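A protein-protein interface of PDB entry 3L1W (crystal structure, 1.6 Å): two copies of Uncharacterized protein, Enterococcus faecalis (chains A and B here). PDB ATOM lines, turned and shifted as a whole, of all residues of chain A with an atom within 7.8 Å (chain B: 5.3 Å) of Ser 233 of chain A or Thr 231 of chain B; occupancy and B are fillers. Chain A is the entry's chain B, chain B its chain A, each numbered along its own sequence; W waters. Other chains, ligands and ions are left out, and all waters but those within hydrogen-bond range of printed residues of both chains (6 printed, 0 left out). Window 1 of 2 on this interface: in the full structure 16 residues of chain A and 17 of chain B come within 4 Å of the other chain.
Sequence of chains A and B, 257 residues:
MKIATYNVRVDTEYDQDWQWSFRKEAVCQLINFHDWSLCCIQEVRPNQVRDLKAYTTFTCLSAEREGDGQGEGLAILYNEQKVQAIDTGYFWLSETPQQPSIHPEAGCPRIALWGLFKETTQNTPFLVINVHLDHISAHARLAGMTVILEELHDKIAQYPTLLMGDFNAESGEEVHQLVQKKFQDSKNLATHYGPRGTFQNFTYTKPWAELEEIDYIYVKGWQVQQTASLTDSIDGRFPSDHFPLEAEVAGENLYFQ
N of Trp 208 of chain B sits at hydrogen-bond distance from OD2 of Asp 235 of chain A, 2.9 Å away.
The side-chain hydroxyl (OH) of Tyr 193 of chain A sits at hydrogen-bond distance from the side-chain carboxylate (OD2) of Asp 232 of chain B (2.6 Å).
Among the printed residues, pairs that only touch across the chains: Tyr 204 of chain A with Phe 238 of chain B (3.9 Å), Thr 231 of chain A with Ser 233 of chain B (3.7 Å), Ser 233 of chain A with Trp 208 of chain B (3.3 Å), Ser 233 of chain A with Thr 231 of chain B (3.7 Å) and Ile 234 of chain A with Trp 208 of chain B (3.7 Å).
Printed residues of chain B within 4 Å of Tyr 193 of chain A: Asp 232 (2.6 Å).
Printed residues of chain B within 4 Å of Tyr 204 of chain A: Phe 238 (3.9 Å).
Of the printed residues of chain B, Asp 235 of chain A touches Trp 208.
Of the printed residues of chain A, Thr 231 of chain B touches Ser 233.
The nearest printed residue of chain B that does not touch Ser 233 of chain A is Pro 195 of chain B (6.1 Å).
The nearest residue of chain A that does not touch Thr 231 of chain B is Asp 232 of chain A (4.2 Å).
The nearest printed residue of chain B that does not touch Thr 231 of chain A is Asp 232 of chain B (4.2 Å).
Printed residues of chain B that touch a printed residue of chain A: Trp 208, Thr 231, Asp 232, Ser 233 and Phe 238.
Of the 16 printed residues of chain A, 6 touch a printed residue of chain B.
Printed residues of chain A that touch a printed residue of chain B: Tyr 193, Tyr 204, Thr 231, Ser 233, Ile 234 and Asp 235.
Hydrophobic or aromatic side chains of chain A that line the printed part of chain B: Tyr 193, Tyr 204 and Ile 234.
Among the printed residues, 7 pairs touch across the chains.
Thr 231 of chain A touches Ser 233 of chain B, and with the chains exchanged Ser 233 of chain A touches Thr 231 of chain B.
6 positions are printed for both chains.
Of the 7 pairs that touch across the chains among the printed residues, 2 have their exchanged pair printed and touching as well.
Water W2 lies within hydrogen-bond range of the side-chain hydroxyl of Ser 233 of chain B (2.6 Å), the backbone carbonyl oxygen of Thr 231 of chain B (2.6 Å) and the side-chain hydroxyl of Thr 231 of chain A (3.0 Å).
Water W4 lies within hydrogen-bond range of OG of Ser 233 of chain A (2.6 Å), O of Thr 231 of chain A (2.7 Å) and OG1 of Thr 231 of chain B (2.9 Å).
Water W3 lies within hydrogen-bond range of the side-chain carboxylate (OD1) of Asp 235 of chain A and the backbone NH (N) of Trp 208 of chain B.
Water W5 lies within hydrogen-bond range of the side-chain hydroxyl of Ser 233 of chain A (2.8 Å), the backbone NH of Gly 236 of chain A (2.9 Å), the indole nitrogen of Trp 208 of chain B (3.2 Å) and the side-chain hydroxyl of Tyr 204 of chain A (3.2 Å).
Water W1 bridges OG of Ser 233 of chain B (2.9 Å) and O of Thr 231 of chain A (3.5 Å).
Water W6 lies within hydrogen-bond range of the backbone NH (N) of Asp 232 of chain A (3.2 Å), the backbone NH (N) of Asp 232 of chain B (3.2 Å), the side-chain hydroxyl (OG1) of Thr 231 of chain B (3.2 Å) and the side-chain hydroxyl (OG1) of Thr 231 of chain A (3.4 Å).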
ATOM      1  N   TRP A  18       7.218  24.242 -17.595  1.00  0.00           N
ATOM      2  CA  TRP A  18       8.421  23.473 -17.303  1.00  0.00           C
ATOM      3  C   TRP A  18       9.480  23.763 -18.367  1.00  0.00           C
ATOM      4  O   TRP A  18      10.346  22.936 -18.644  1.00  0.00           O
ATOM      5  CB  TRP A  18       8.091  21.976 -17.196  1.00  0.00           C
ATOM      6  CG  TRP A  18       9.039  21.179 -16.324  1.00  0.00           C
ATOM      7  CD1 TRP A  18       9.587  19.966 -16.618  1.00  0.00           C
ATOM      8  CD2 TRP A  18       9.540  21.542 -15.025  1.00  0.00           C
ATOM      9  NE1 TRP A  18      10.399  19.548 -15.583  1.00  0.00           N
ATOM     10  CE2 TRP A  18      10.383  20.500 -14.596  1.00  0.00           C
ATOM     11  CE3 TRP A  18       9.349  22.646 -14.183  1.00  0.00           C
ATOM     12  CZ2 TRP A  18      11.053  20.533 -13.366  1.00  0.00           C
ATOM     13  CZ3 TRP A  18      10.012  22.675 -12.962  1.00  0.00           C
ATOM     14  CH2 TRP A  18      10.851  21.625 -12.567  1.00  0.00           C
ATOM     15  N   ALA A  26      17.172  23.573 -10.762  1.00  0.00           N
ATOM     16  CA  ALA A  26      17.226  22.144 -10.478  1.00  0.00           C
ATOM     17  C   ALA A  26      18.318  21.457 -11.279  1.00  0.00           C
ATOM     18  O   ALA A  26      19.027  20.595 -10.765  1.00  0.00           O
ATOM     19  CB  ALA A  26      15.880  21.484 -10.743  1.00  0.00           C
ATOM     20  N   LEU A  30      21.744  19.987  -9.550  1.00  0.00           N
ATOM     21  CA  LEU A  30      22.080  18.575  -9.744  1.00  0.00           C
ATOM     22  C   LEU A  30      23.536  18.446 -10.160  1.00  0.00           C
ATOM     23  O   LEU A  30      24.297  17.663  -9.586  1.00  0.00           O
ATOM     24  CB  LEU A  30      21.157  17.929 -10.795  1.00  0.00           C
ATOM     25  CG  LEU A  30      21.281  16.423 -11.073  1.00  0.00           C
ATOM     26  CD1 LEU A  30      19.989  15.937 -11.738  1.00  0.00           C
ATOM     27  CD2 LEU A  30      22.472  16.056 -11.962  1.00  0.00           C
ATOM     28  N   TYR A 193      24.065   1.260 -11.604  1.00  0.00           N
ATOM     29  CA  TYR A 193      23.084   1.677 -10.600  1.00  0.00           C
ATOM     30  C   TYR A 193      21.998   2.493 -11.274  1.00  0.00           C
ATOM     31  O   TYR A 193      22.290   3.351 -12.107  1.00  0.00           O
ATOM     32  CB  TYR A 193      23.772   2.502  -9.505  1.00  0.00           C
ATOM     33  CG  TYR A 193      22.854   2.948  -8.386  1.00  0.00           C
ATOM     34  CD1 TYR A 193      22.243   2.024  -7.554  1.00  0.00           C
ATOM     35  CD2 TYR A 193      22.622   4.302  -8.153  1.00  0.00           C
ATOM     36  CE1 TYR A 193      21.406   2.433  -6.523  1.00  0.00           C
ATOM     37  CE2 TYR A 193      21.785   4.723  -7.129  1.00  0.00           C
ATOM     38  CZ  TYR A 193      21.185   3.787  -6.318  1.00  0.00           C
ATOM     39  OH  TYR A 193      20.347   4.181  -5.301  1.00  0.00           O
ATOM     40  N   TYR A 204       7.263  11.539 -14.565  1.00  0.00           N
ATOM     41  CA  TYR A 204       7.827  11.163 -13.273  1.00  0.00           C
ATOM     42  C   TYR A 204       7.528   9.697 -12.956  1.00  0.00           C
ATOM     43  O   TYR A 204       8.348   9.000 -12.362  1.00  0.00           O
ATOM     44  CB  TYR A 204       7.263  12.090 -12.193  1.00  0.00           C
ATOM     45  CG  TYR A 204       7.755  11.810 -10.783  1.00  0.00           C
ATOM     46  CD1 TYR A 204       9.085  12.003 -10.443  1.00  0.00           C
ATOM     47  CD2 TYR A 204       6.877  11.382  -9.797  1.00  0.00           C
ATOM     48  CE1 TYR A 204       9.538  11.760  -9.158  1.00  0.00           C
ATOM     49  CE2 TYR A 204       7.318  11.136  -8.506  1.00  0.00           C
ATOM     50  CZ  TYR A 204       8.650  11.329  -8.197  1.00  0.00           C
ATOM     51  OH  TYR A 204       9.107  11.089  -6.922  1.00  0.00           O
ATOM     52  N   LEU A 230      20.962   8.639 -13.159  1.00  0.00           N
ATOM     53  CA  LEU A 230      20.618   9.388 -11.952  1.00  0.00           C
ATOM     54  C   LEU A 230      19.164   9.865 -11.984  1.00  0.00           C
ATOM     55  O   LEU A 230      18.770  10.625 -12.869  1.00  0.00           O
ATOM     56  CB  LEU A 230      21.575  10.577 -11.791  1.00  0.00           C
ATOM     57  CG  LEU A 230      23.064  10.210 -11.817  1.00  0.00           C
ATOM     58  CD1 LEU A 230      23.941  11.459 -11.696  1.00  0.00           C
ATOM     59  CD2 LEU A 230      23.413   9.202 -10.703  1.00  0.00           C
ATOM     60  N   THR A 231      18.370   9.408 -11.021  1.00  0.00           N
ATOM     61  CA  THR A 231      16.930   9.680 -11.025  1.00  0.00           C
ATOM     62  C   THR A 231      16.514  10.857 -10.147  1.00  0.00           C
ATOM     63  O   THR A 231      15.354  10.947  -9.727  1.00  0.00           O
ATOM     64  CB  THR A 231      16.129   8.416 -10.605  1.00  0.00           C
ATOM     65  OG1 THR A 231      16.489   8.041  -9.275  1.00  0.00           O
ATOM     66  CG2 THR A 231      16.450   7.263 -11.552  1.00  0.00           C
ATOM     67  N   ASP A 232      17.463  11.749  -9.863  1.00  0.00           N
ATOM     68  CA  ASP A 232      17.187  12.955  -9.076  1.00  0.00           C
ATOM     69  C   ASP A 232      15.916  13.630  -9.559  1.00  0.00           C
ATOM     70  O   ASP A 232      15.726  13.820 -10.764  1.00  0.00           O
ATOM     71  CB  ASP A 232      18.319  13.973  -9.221  1.00  0.00           C
ATOM     72  CG  ASP A 232      19.661  13.441  -8.773  1.00  0.00           C
ATOM     73  OD1 ASP A 232      19.956  12.259  -9.022  1.00  0.00           O
ATOM     74  OD2 ASP A 232      20.437  14.216  -8.181  1.00  0.00           O
ATOM     75  N   SER A 233      15.063  14.031  -8.623  1.00  0.00           N
ATOM     76  CA  SER A 233      13.838  14.712  -8.985  1.00  0.00           C
ATOM     77  C   SER A 233      13.741  16.032  -8.255  1.00  0.00           C
ATOM     78  O   SER A 233      14.506  16.305  -7.326  1.00  0.00           O
ATOM     79  CB  SER A 233      12.612  13.854  -8.652  1.00  0.00           C
ATOM     80  OG  SER A 233      12.581  13.536  -7.266  1.00  0.00           O
ATOM     81  N   ILE A 234      12.796  16.851  -8.688  1.00  0.00           N
ATOM     82  CA  ILE A 234      12.488  18.095  -8.000  1.00  0.00           C
ATOM     83  C   ILE A 234      10.976  18.122  -7.779  1.00  0.00           C
ATOM     84  O   ILE A 234      10.209  18.431  -8.685  1.00  0.00           O
ATOM     85  CB  ILE A 234      13.000  19.331  -8.804  1.00  0.00           C
ATOM     86  CG1 ILE A 234      12.450  20.634  -8.223  1.00  0.00           C
ATOM     87  CG2 ILE A 234      12.664  19.213 -10.299  1.00  0.00           C
ATOM     88  CD1 ILE A 234      12.846  20.872  -6.778  1.00  0.00           C
ATOM     89  N   ASP A 235      10.560  17.739  -6.576  1.00  0.00           N
ATOM     90  CA  ASP A 235       9.145  17.716  -6.182  1.00  0.00           C
ATOM     91  C   ASP A 235       8.186  17.160  -7.245  1.00  0.00           C
ATOM     92  O   ASP A 235       7.260  17.838  -7.672  1.00  0.00           O
ATOM     93  CB  ASP A 235       8.680  19.109  -5.735  1.00  0.00           C
ATOM     94  CG  ASP A 235       7.398  19.069  -4.917  1.00  0.00           C
ATOM     95  OD1 ASP A 235       6.873  20.153  -4.598  1.00  0.00           O
ATOM     96  OD2 ASP A 235       6.901  17.971  -4.587  1.00  0.00           O
ATOM     97  N   GLY A 236       8.400  15.915  -7.653  1.00  0.00           N
ATOM     98  CA  GLY A 236       7.447  15.242  -8.516  1.00  0.00           C
ATOM     99  C   GLY A 236       7.661  15.503  -9.992  1.00  0.00           C
ATOM    100  O   GLY A 236       6.834  15.115 -10.819  1.00  0.00           O
ATOM    101  N   ARG A 237       8.765  16.166 -10.323  1.00  0.00           N
ATOM    102  CA  ARG A 237       9.165  16.363 -11.719  1.00  0.00           C
ATOM    103  C   ARG A 237      10.635  16.009 -11.880  1.00  0.00           C
ATOM    104  O   ARG A 237      11.370  15.953 -10.900  1.00  0.00           O
ATOM    105  CB  ARG A 237       8.971  17.820 -12.136  1.00  0.00           C
ATOM    106  CG  ARG A 237       7.529  18.295 -12.153  1.00  0.00           C
ATOM    107  CD  ARG A 237       7.453  19.766 -12.559  1.00  0.00           C
ATOM    108  NE  ARG A 237       6.094  20.289 -12.481  1.00  0.00           N
ATOM    109  CZ  ARG A 237       5.453  20.873 -13.490  1.00  0.00           C
ATOM    110  NH1 ARG A 237       6.046  21.019 -14.667  1.00  0.00           N
ATOM    111  NH2 ARG A 237       4.214  21.314 -13.321  1.00  0.00           N
ATOM    112  N   PHE A 238      11.069  15.771 -13.113  1.00  0.00           N
ATOM    113  CA  PHE A 238      12.488  15.576 -13.372  1.00  0.00           C
ATOM    114  C   PHE A 238      13.033  16.864 -13.956  1.00  0.00           C
ATOM    115  O   PHE A 238      12.328  17.547 -14.694  1.00  0.00           O
ATOM    116  CB  PHE A 238      12.728  14.410 -14.331  1.00  0.00           C
ATOM    117  CG  PHE A 238      12.383  13.064 -13.751  1.00  0.00           C
ATOM    118  CD1 PHE A 238      12.954  12.637 -12.561  1.00  0.00           C
ATOM    119  CD2 PHE A 238      11.501  12.210 -14.414  1.00  0.00           C
ATOM    120  CE1 PHE A 238      12.645  11.388 -12.029  1.00  0.00           C
ATOM    121  CE2 PHE A 238      11.186  10.962 -13.889  1.00  0.00           C
ATOM    122  CZ  PHE A 238      11.760  10.549 -12.698  1.00  0.00           C
ATOM    123  N   PRO A 239      14.285  17.205 -13.619  1.00  0.00           N
ATOM    124  CA  PRO A 239      14.857  18.476 -14.081  1.00  0.00           C
ATOM    125  C   PRO A 239      15.042  18.522 -15.598  1.00  0.00           C
ATOM    126  O   PRO A 239      14.992  19.600 -16.166  1.00  0.00           O
ATOM    127  CB  PRO A 239      16.218  18.543 -13.357  1.00  0.00           C
ATOM    128  CG  PRO A 239      16.078  17.609 -12.181  1.00  0.00           C
ATOM    129  CD  PRO A 239      15.181  16.497 -12.689  1.00  0.00           C
ATOM    130  N   PHE A 243      17.560  11.360 -17.839  1.00  0.00           N
ATOM    131  CA  PHE A 243      18.389  11.261 -16.632  1.00  0.00           C
ATOM    132  C   PHE A 243      19.837  11.526 -17.039  1.00  0.00           C
ATOM    133  O   PHE A 243      20.258  11.167 -18.139  1.00  0.00           O
ATOM    134  CB  PHE A 243      18.307   9.853 -16.032  1.00  0.00           C
ATOM    135  CG  PHE A 243      16.932   9.447 -15.592  1.00  0.00           C
ATOM    136  CD1 PHE A 243      16.138  10.314 -14.859  1.00  0.00           C
ATOM    137  CD2 PHE A 243      16.459   8.169 -15.855  1.00  0.00           C
ATOM    138  CE1 PHE A 243      14.874   9.922 -14.427  1.00  0.00           C
ATOM    139  CE2 PHE A 243      15.196   7.771 -15.431  1.00  0.00           C
ATOM    140  CZ  PHE A 243      14.407   8.642 -14.713  1.00  0.00           C
ATOM    141  N   PRO B 195      14.936  17.583  -0.880  1.00  0.00           N
ATOM    142  CA  PRO B 195      13.922  18.094   0.046  1.00  0.00           C
ATOM    143  C   PRO B 195      14.484  18.270   1.458  1.00  0.00           C
ATOM    144  O   PRO B 195      15.396  17.539   1.851  1.00  0.00           O
ATOM    145  CB  PRO B 195      12.851  16.999   0.019  1.00  0.00           C
ATOM    146  CG  PRO B 195      13.598  15.746  -0.310  1.00  0.00           C
ATOM    147  CD  PRO B 195      14.704  16.176  -1.259  1.00  0.00           C
ATOM    148  N   TRP B 208       6.731  17.491  -1.751  1.00  0.00           N
ATOM    149  CA  TRP B 208       7.819  17.768  -0.823  1.00  0.00           C
ATOM    150  C   TRP B 208       7.364  18.546   0.416  1.00  0.00           C
ATOM    151  O   TRP B 208       7.872  18.317   1.519  1.00  0.00           O
ATOM    152  CB  TRP B 208       8.980  18.449  -1.547  1.00  0.00           C
ATOM    153  CG  TRP B 208       9.789  17.482  -2.375  1.00  0.00           C
ATOM    154  CD1 TRP B 208       9.470  16.181  -2.668  1.00  0.00           C
ATOM    155  CD2 TRP B 208      11.049  17.736  -3.011  1.00  0.00           C
ATOM    156  NE1 TRP B 208      10.455  15.616  -3.448  1.00  0.00           N
ATOM    157  CE2 TRP B 208      11.436  16.545  -3.667  1.00  0.00           C
ATOM    158  CE3 TRP B 208      11.891  18.849  -3.084  1.00  0.00           C
ATOM    159  CZ2 TRP B 208      12.627  16.441  -4.389  1.00  0.00           C
ATOM    160  CZ3 TRP B 208      13.074  18.742  -3.806  1.00  0.00           C
ATOM    161  CH2 TRP B 208      13.427  17.549  -4.444  1.00  0.00           C
ATOM    162  N   SER B 229      19.212  15.371   1.002  1.00  0.00           N
ATOM    163  CA  SER B 229      18.254  14.284   1.184  1.00  0.00           C
ATOM    164  C   SER B 229      18.196  13.552  -0.151  1.00  0.00           C
ATOM    165  O   SER B 229      17.953  14.177  -1.185  1.00  0.00           O
ATOM    166  CB  SER B 229      16.869  14.827   1.534  1.00  0.00           C
ATOM    167  OG  SER B 229      16.864  15.414   2.827  1.00  0.00           O
ATOM    168  N   LEU B 230      18.408  12.238  -0.135  1.00  0.00           N
ATOM    169  CA  LEU B 230      18.602  11.483  -1.377  1.00  0.00           C
ATOM    170  C   LEU B 230      17.303  10.816  -1.831  1.00  0.00           C
ATOM    171  O   LEU B 230      16.733  10.005  -1.113  1.00  0.00           O
ATOM    172  CB  LEU B 230      19.693  10.423  -1.164  1.00  0.00           C
ATOM    173  CG  LEU B 230      21.015  11.011  -0.653  1.00  0.00           C
ATOM    174  CD1 LEU B 230      22.035   9.915  -0.384  1.00  0.00           C
ATOM    175  CD2 LEU B 230      21.573  12.032  -1.660  1.00  0.00           C
ATOM    176  N   THR B 231      16.829  11.176  -3.023  1.00  0.00           N
ATOM    177  CA  THR B 231      15.519  10.718  -3.499  1.00  0.00           C
ATOM    178  C   THR B 231      15.596   9.519  -4.444  1.00  0.00           C
ATOM    179  O   THR B 231      14.677   9.277  -5.233  1.00  0.00           O
ATOM    180  CB  THR B 231      14.723  11.871  -4.179  1.00  0.00           C
ATOM    181  OG1 THR B 231      15.436  12.341  -5.327  1.00  0.00           O
ATOM    182  CG2 THR B 231      14.533  13.040  -3.197  1.00  0.00           C
ATOM    183  N   ASP B 232      16.693   8.769  -4.360  1.00  0.00           N
ATOM    184  CA  ASP B 232      16.857   7.550  -5.158  1.00  0.00           C
ATOM    185  C   ASP B 232      15.592   6.705  -5.130  1.00  0.00           C
ATOM    186  O   ASP B 232      14.996   6.483  -4.066  1.00  0.00           O
ATOM    187  CB  ASP B 232      17.992   6.689  -4.604  1.00  0.00           C
ATOM    188  CG  ASP B 232      19.317   7.410  -4.551  1.00  0.00           C
ATOM    189  OD1 ASP B 232      19.339   8.619  -4.224  1.00  0.00           O
ATOM    190  OD2 ASP B 232      20.349   6.752  -4.811  1.00  0.00           O
ATOM    191  N   SER B 233      15.197   6.194  -6.292  1.00  0.00           N
ATOM    192  CA  SER B 233      14.008   5.365  -6.357  1.00  0.00           C
ATOM    193  C   SER B 233      14.345   4.055  -7.046  1.00  0.00           C
ATOM    194  O   SER B 233      15.413   3.906  -7.634  1.00  0.00           O
ATOM    195  CB  SER B 233      12.886   6.077  -7.124  1.00  0.00           C
ATOM    196  OG  SER B 233      13.317   6.439  -8.431  1.00  0.00           O
ATOM    197  N   PHE B 238      10.157   3.874  -3.433  1.00  0.00           N
ATOM    198  CA  PHE B 238      11.355   4.251  -2.703  1.00  0.00           C
ATOM    199  C   PHE B 238      11.825   3.029  -1.941  1.00  0.00           C
ATOM    200  O   PHE B 238      11.000   2.250  -1.464  1.00  0.00           O
ATOM    201  CB  PHE B 238      11.070   5.401  -1.742  1.00  0.00           C
ATOM    202  CG  PHE B 238      10.768   6.705  -2.430  1.00  0.00           C
ATOM    203  CD1 PHE B 238      11.657   7.246  -3.355  1.00  0.00           C
ATOM    204  CD2 PHE B 238       9.606   7.409  -2.126  1.00  0.00           C
ATOM    205  CE1 PHE B 238      11.375   8.467  -3.984  1.00  0.00           C
ATOM    206  CE2 PHE B 238       9.322   8.623  -2.742  1.00  0.00           C
ATOM    207  CZ  PHE B 238      10.205   9.154  -3.666  1.00  0.00           C
ATOM    208  N   PHE B 243      13.943   8.940   3.141  1.00  0.00           N
ATOM    209  CA  PHE B 243      15.120   9.185   2.300  1.00  0.00           C
ATOM    210  C   PHE B 243      16.357   9.130   3.187  1.00  0.00           C
ATOM    211  O   PHE B 243      16.314   9.568   4.335  1.00  0.00           O
ATOM    212  CB  PHE B 243      15.075  10.591   1.692  1.00  0.00           C
ATOM    213  CG  PHE B 243      13.917  10.828   0.772  1.00  0.00           C
ATOM    214  CD1 PHE B 243      13.557   9.869  -0.160  1.00  0.00           C
ATOM    215  CD2 PHE B 243      13.209  12.027   0.814  1.00  0.00           C
ATOM    216  CE1 PHE B 243      12.492  10.093  -1.033  1.00  0.00           C
ATOM    217  CE2 PHE B 243      12.150  12.263  -0.060  1.00  0.00           C
ATOM    218  CZ  PHE B 243      11.789  11.294  -0.981  1.00  0.00           C
HETATM  219  O   HOH W   1      12.519   8.979  -9.687  1.00  0.00           O
HETATM  220  O   HOH W   2      14.008   8.821  -7.741  1.00  0.00           O
HETATM  221  O   HOH W   3       5.451  20.405  -2.377  1.00  0.00           O
HETATM  222  O   HOH W   4      13.871  11.238  -7.518  1.00  0.00           O
HETATM  223  O   HOH W   5      10.071  14.074  -6.189  1.00  0.00           O
HETATM  224  O   HOH W   6      17.269  10.390  -7.015  1.00  0.00           O
